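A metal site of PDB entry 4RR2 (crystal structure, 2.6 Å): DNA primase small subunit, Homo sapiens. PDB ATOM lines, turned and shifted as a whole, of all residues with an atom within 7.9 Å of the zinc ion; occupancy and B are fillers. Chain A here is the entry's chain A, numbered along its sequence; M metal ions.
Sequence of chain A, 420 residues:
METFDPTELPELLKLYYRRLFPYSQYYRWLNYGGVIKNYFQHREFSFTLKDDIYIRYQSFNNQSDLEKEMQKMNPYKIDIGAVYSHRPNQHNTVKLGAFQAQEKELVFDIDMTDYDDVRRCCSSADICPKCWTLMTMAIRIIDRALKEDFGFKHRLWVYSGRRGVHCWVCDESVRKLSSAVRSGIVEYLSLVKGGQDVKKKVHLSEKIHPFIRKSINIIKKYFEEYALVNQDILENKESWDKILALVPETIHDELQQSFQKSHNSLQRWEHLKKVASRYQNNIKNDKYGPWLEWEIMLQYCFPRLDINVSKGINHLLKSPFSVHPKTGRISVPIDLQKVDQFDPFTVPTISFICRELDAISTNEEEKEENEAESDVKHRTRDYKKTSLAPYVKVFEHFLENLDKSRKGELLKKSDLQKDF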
ATOM      1  N   MET A 112      -2.800 -29.349 -12.301  1.00  0.00           N
ATOM      2  CA  MET A 112      -2.768 -27.938 -12.002  1.00  0.00           C
ATOM      3  C   MET A 112      -2.371 -27.075 -13.198  1.00  0.00           C
ATOM      4  O   MET A 112      -2.864 -25.952 -13.334  1.00  0.00           O
ATOM      5  CB  MET A 112      -1.814 -27.688 -10.806  1.00  0.00           C
ATOM      6  CG  MET A 112      -2.074 -26.406 -10.040  1.00  0.00           C
ATOM      7  SD  MET A 112      -3.759 -26.334  -9.345  1.00  0.00           S
ATOM      8  CE  MET A 112      -3.560 -27.341  -7.885  1.00  0.00           C
ATOM      9  N   ARG A 119      -4.490 -18.869 -11.739  1.00  0.00           N
ATOM     10  CA  ARG A 119      -3.727 -18.885 -10.495  1.00  0.00           C
ATOM     11  C   ARG A 119      -2.600 -17.867 -10.534  1.00  0.00           C
ATOM     12  O   ARG A 119      -1.930 -17.718 -11.539  1.00  0.00           O
ATOM     13  CB  ARG A 119      -3.200 -20.305 -10.214  1.00  0.00           C
ATOM     14  CG  ARG A 119      -2.420 -20.939 -11.383  1.00  0.00           C
ATOM     15  CD  ARG A 119      -2.401 -22.468 -11.287  1.00  0.00           C
ATOM     16  NE  ARG A 119      -1.559 -22.913 -10.193  1.00  0.00           N
ATOM     17  CZ  ARG A 119      -0.407 -23.559 -10.357  1.00  0.00           C
ATOM     18  NH1 ARG A 119       0.040 -23.836 -11.580  1.00  0.00           N
ATOM     19  NH2 ARG A 119       0.306 -23.877  -9.297  1.00  0.00           N
ATOM     20  N   ARG A 120      -2.405 -17.161  -9.419  1.00  0.00           N
ATOM     21  CA  ARG A 120      -1.380 -16.113  -9.284  1.00  0.00           C
ATOM     22  C   ARG A 120      -0.292 -16.534  -8.322  1.00  0.00           C
ATOM     23  O   ARG A 120       0.714 -15.850  -8.202  1.00  0.00           O
ATOM     24  CB  ARG A 120      -2.008 -14.825  -8.753  1.00  0.00           C
ATOM     25  CG  ARG A 120      -2.777 -13.990  -9.773  1.00  0.00           C
ATOM     26  CD  ARG A 120      -3.905 -13.198  -9.107  1.00  0.00           C
ATOM     27  NE  ARG A 120      -3.471 -12.455  -7.918  1.00  0.00           N
ATOM     28  CZ  ARG A 120      -2.747 -11.344  -7.950  1.00  0.00           C
ATOM     29  NH1 ARG A 120      -2.366 -10.829  -9.106  1.00  0.00           N
ATOM     30  NH2 ARG A 120      -2.396 -10.748  -6.818  1.00  0.00           N
ATOM     31  N   CYS A 121      -0.509 -17.645  -7.637  1.00  0.00           N
ATOM     32  CA  CYS A 121       0.452 -18.134  -6.659  1.00  0.00           C
ATOM     33  C   CYS A 121       1.766 -18.624  -7.235  1.00  0.00           C
ATOM     34  O   CYS A 121       2.767 -17.928  -7.188  1.00  0.00           O
ATOM     35  CB  CYS A 121      -0.182 -19.238  -5.836  1.00  0.00           C
ATOM     36  SG  CYS A 121      -0.928 -20.572  -6.819  1.00  0.00           S
ATOM     37  N   CYS A 122       1.769 -19.833  -7.794  1.00  0.00           N
ATOM     38  CA  CYS A 122       2.999 -20.390  -8.343  1.00  0.00           C
ATOM     39  C   CYS A 122       3.156 -20.275  -9.855  1.00  0.00           C
ATOM     40  O   CYS A 122       2.413 -19.564 -10.543  1.00  0.00           O
ATOM     41  CB  CYS A 122       3.117 -21.883  -8.015  1.00  0.00           C
ATOM     42  SG  CYS A 122       2.158 -22.458  -6.681  1.00  0.00           S
ATOM     43  N   SER A 123       4.132 -21.056 -10.335  1.00  0.00           N
ATOM     44  CA  SER A 123       4.513 -21.212 -11.739  1.00  0.00           C
ATOM     45  C   SER A 123       3.906 -22.546 -12.181  1.00  0.00           C
ATOM     46  O   SER A 123       3.580 -23.388 -11.342  1.00  0.00           O
ATOM     47  CB  SER A 123       6.023 -21.316 -11.820  1.00  0.00           C
ATOM     48  OG  SER A 123       6.442 -22.336 -10.929  1.00  0.00           O
ATOM     49  N   ASP A 126       4.561 -26.190 -10.716  1.00  0.00           N
ATOM     50  CA  ASP A 126       4.564 -26.191  -9.263  1.00  0.00           C
ATOM     51  C   ASP A 126       3.194 -26.046  -8.631  1.00  0.00           C
ATOM     52  O   ASP A 126       2.192 -25.816  -9.307  1.00  0.00           O
ATOM     53  CB  ASP A 126       5.464 -25.089  -8.734  1.00  0.00           C
ATOM     54  CG  ASP A 126       6.889 -25.262  -9.166  1.00  0.00           C
ATOM     55  OD1 ASP A 126       7.407 -26.400  -9.073  1.00  0.00           O
ATOM     56  OD2 ASP A 126       7.481 -24.257  -9.613  1.00  0.00           O
ATOM     57  N   ILE A 127       3.152 -26.223  -7.319  1.00  0.00           N
ATOM     58  CA  ILE A 127       1.924 -26.095  -6.558  1.00  0.00           C
ATOM     59  C   ILE A 127       2.248 -25.650  -5.152  1.00  0.00           C
ATOM     60  O   ILE A 127       3.311 -25.938  -4.630  1.00  0.00           O
ATOM     61  CB  ILE A 127       1.161 -27.427  -6.429  1.00  0.00           C
ATOM     62  CG1 ILE A 127       2.029 -28.469  -5.726  1.00  0.00           C
ATOM     63  CG2 ILE A 127       0.712 -27.896  -7.782  1.00  0.00           C
ATOM     64  CD1 ILE A 127       1.228 -29.564  -5.093  1.00  0.00           C
ATOM     65  N   CYS A 128       1.329 -24.935  -4.532  1.00  0.00           N
ATOM     66  CA  CYS A 128       1.578 -24.514  -3.176  1.00  0.00           C
ATOM     67  C   CYS A 128       0.277 -24.637  -2.412  1.00  0.00           C
ATOM     68  O   CYS A 128      -0.731 -25.057  -2.966  1.00  0.00           O
ATOM     69  CB  CYS A 128       2.061 -23.076  -3.164  1.00  0.00           C
ATOM     70  SG  CYS A 128       0.856 -21.987  -3.823  1.00  0.00           S
ATOM     71  N   PRO A 129       0.281 -24.305  -1.130  1.00  0.00           N
ATOM     72  CA  PRO A 129      -0.981 -24.434  -0.425  1.00  0.00           C
ATOM     73  C   PRO A 129      -2.060 -23.473  -0.956  1.00  0.00           C
ATOM     74  O   PRO A 129      -3.248 -23.700  -0.765  1.00  0.00           O
ATOM     75  CB  PRO A 129      -0.579 -24.156   1.016  1.00  0.00           C
ATOM     76  CG  PRO A 129       0.857 -24.637   1.073  1.00  0.00           C
ATOM     77  CD  PRO A 129       1.395 -24.054  -0.193  1.00  0.00           C
ATOM     78  N   LYS A 130      -1.637 -22.413  -1.640  1.00  0.00           N
ATOM     79  CA  LYS A 130      -2.609 -21.451  -2.157  1.00  0.00           C
ATOM     80  C   LYS A 130      -3.395 -21.904  -3.369  1.00  0.00           C
ATOM     81  O   LYS A 130      -4.468 -21.366  -3.633  1.00  0.00           O
ATOM     82  CB  LYS A 130      -1.927 -20.129  -2.465  1.00  0.00           C
ATOM     83  CG  LYS A 130      -1.399 -19.402  -1.245  1.00  0.00           C
ATOM     84  CD  LYS A 130      -0.978 -17.999  -1.646  1.00  0.00           C
ATOM     85  CE  LYS A 130      -0.122 -17.354  -0.609  1.00  0.00           C
ATOM     86  NZ  LYS A 130       0.528 -16.153  -1.187  1.00  0.00           N
ATOM     87  N   CYS A 131      -2.855 -22.864  -4.124  1.00  0.00           N
ATOM     88  CA  CYS A 131      -3.576 -23.354  -5.301  1.00  0.00           C
ATOM     89  C   CYS A 131      -4.133 -24.753  -5.141  1.00  0.00           C
ATOM     90  O   CYS A 131      -4.993 -25.168  -5.926  1.00  0.00           O
ATOM     91  CB  CYS A 131      -2.703 -23.264  -6.562  1.00  0.00           C
ATOM     92  SG  CYS A 131      -1.011 -23.875  -6.493  1.00  0.00           S
ATOM     93  N   TRP A 132      -3.682 -25.477  -4.120  1.00  0.00           N
ATOM     94  CA  TRP A 132      -4.158 -26.833  -3.935  1.00  0.00           C
ATOM     95  C   TRP A 132      -5.638 -26.949  -3.666  1.00  0.00           C
ATOM     96  O   TRP A 132      -6.202 -28.028  -3.791  1.00  0.00           O
ATOM     97  CB  TRP A 132      -3.417 -27.536  -2.805  1.00  0.00           C
ATOM     98  CG  TRP A 132      -3.768 -28.988  -2.752  1.00  0.00           C
ATOM     99  CD1 TRP A 132      -4.614 -29.613  -1.876  1.00  0.00           C
ATOM    100  CD2 TRP A 132      -3.316 -30.005  -3.659  1.00  0.00           C
ATOM    101  NE1 TRP A 132      -4.723 -30.954  -2.185  1.00  0.00           N
ATOM    102  CE2 TRP A 132      -3.942 -31.218  -3.273  1.00  0.00           C
ATOM    103  CE3 TRP A 132      -2.455 -30.008  -4.760  1.00  0.00           C
ATOM    104  CZ2 TRP A 132      -3.726 -32.410  -3.953  1.00  0.00           C
ATOM    105  CZ3 TRP A 132      -2.231 -31.200  -5.433  1.00  0.00           C
ATOM    106  CH2 TRP A 132      -2.863 -32.380  -5.029  1.00  0.00           C
ATOM    107  N   LEU A 134      -7.882 -25.929  -5.429  1.00  0.00           N
ATOM    108  CA  LEU A 134      -8.487 -26.279  -6.707  1.00  0.00           C
ATOM    109  C   LEU A 134      -8.614 -27.818  -6.794  1.00  0.00           C
ATOM    110  O   LEU A 134      -9.669 -28.358  -7.161  1.00  0.00           O
ATOM    111  CB  LEU A 134      -7.644 -25.714  -7.848  1.00  0.00           C
ATOM    112  CG  LEU A 134      -7.515 -24.200  -8.079  1.00  0.00           C
ATOM    113  CD1 LEU A 134      -6.532 -23.954  -9.193  1.00  0.00           C
ATOM    114  CD2 LEU A 134      -8.864 -23.555  -8.466  1.00  0.00           C
ATOM    115  N   TYR A 226     -10.163 -19.137  -0.825  1.00  0.00           N
ATOM    116  CA  TYR A 226      -9.269 -19.471  -1.913  1.00  0.00           C
ATOM    117  C   TYR A 226      -9.055 -18.343  -2.898  1.00  0.00           C
ATOM    118  O   TYR A 226      -7.923 -17.897  -3.110  1.00  0.00           O
ATOM    119  CB  TYR A 226      -9.767 -20.730  -2.670  1.00  0.00           C
ATOM    120  CG  TYR A 226      -9.166 -20.885  -4.066  1.00  0.00           C
ATOM    121  CD1 TYR A 226      -7.834 -21.252  -4.250  1.00  0.00           C
ATOM    122  CD2 TYR A 226      -9.889 -20.525  -5.194  1.00  0.00           C
ATOM    123  CE1 TYR A 226      -7.232 -21.234  -5.529  1.00  0.00           C
ATOM    124  CE2 TYR A 226      -9.300 -20.505  -6.458  1.00  0.00           C
ATOM    125  CZ  TYR A 226      -7.975 -20.849  -6.623  1.00  0.00           C
ATOM    126  OH  TYR A 226      -7.412 -20.748  -7.881  1.00  0.00           O
ATOM    127  N   GLN A 231      -5.686 -16.307  -3.502  1.00  0.00           N
ATOM    128  CA  GLN A 231      -5.296 -15.874  -4.856  1.00  0.00           C
ATOM    129  C   GLN A 231      -5.361 -14.371  -5.003  1.00  0.00           C
ATOM    130  O   GLN A 231      -4.654 -13.790  -5.824  1.00  0.00           O
ATOM    131  CB  GLN A 231      -6.189 -16.523  -5.927  1.00  0.00           C
ATOM    132  CG  GLN A 231      -5.990 -18.025  -6.130  1.00  0.00           C
ATOM    133  CD  GLN A 231      -4.532 -18.412  -6.320  1.00  0.00           C
ATOM    134  OE1 GLN A 231      -3.833 -17.843  -7.160  1.00  0.00           O
ATOM    135  NE2 GLN A 231      -4.069 -19.375  -5.545  1.00  0.00           N
ATOM    136  N   PHE A 345       2.189 -31.709   0.479  1.00  0.00           N
ATOM    137  CA  PHE A 345       3.514 -31.502   1.030  1.00  0.00           C
ATOM    138  C   PHE A 345       3.930 -32.392   2.185  1.00  0.00           C
ATOM    139  O   PHE A 345       5.112 -32.428   2.530  1.00  0.00           O
ATOM    140  CB  PHE A 345       3.656 -30.015   1.378  1.00  0.00           C
ATOM    141  CG  PHE A 345       3.332 -29.117   0.208  1.00  0.00           C
ATOM    142  CD1 PHE A 345       4.257 -28.909  -0.805  1.00  0.00           C
ATOM    143  CD2 PHE A 345       2.077 -28.511   0.098  1.00  0.00           C
ATOM    144  CE1 PHE A 345       3.928 -28.117  -1.927  1.00  0.00           C
ATOM    145  CE2 PHE A 345       1.749 -27.727  -1.008  1.00  0.00           C
ATOM    146  CZ  PHE A 345       2.681 -27.530  -2.028  1.00  0.00           C
HETATM  147 ZN    ZN M   1       0.200 -21.943  -5.996  1.00  0.00          ZN
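The side-chain sulfur (SG) of Cys 122 sits close to the guanidinium group (NH2) of Arg 119, at 3.5 Å. The backbone NH of Lys 130 sits close to the side-chain sulfur of Cys 128 (3.3 Å). The side-chain sulfur (SG) of Cys 131 lies close to the guanidinium group (NH2) of Arg 119 (3.1 Å). O of Asp 126 lies within hydrogen-bond range of NH2 of Arg 119, at 2.7 Å. The backbone NH of Cys 121 is in hydrogen-bond range of the side-chain amide oxygen of Gln 231, 3.4 Å away.
Merely in contact with the zinc ion: Arg 119.
SG of Cys 121 binds the zinc ion, at 2.0 Å. The zinc ion is bound by the side-chain sulfur (SG) of Cys 122 (2.1 Å). The zinc ion is bound by the side-chain sulfur (SG) of Cys 128, at 2.3 Å. SG of Cys 131 is bound to the zinc ion (2.3 Å). The zinc ion has four donor atoms within binding distance.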
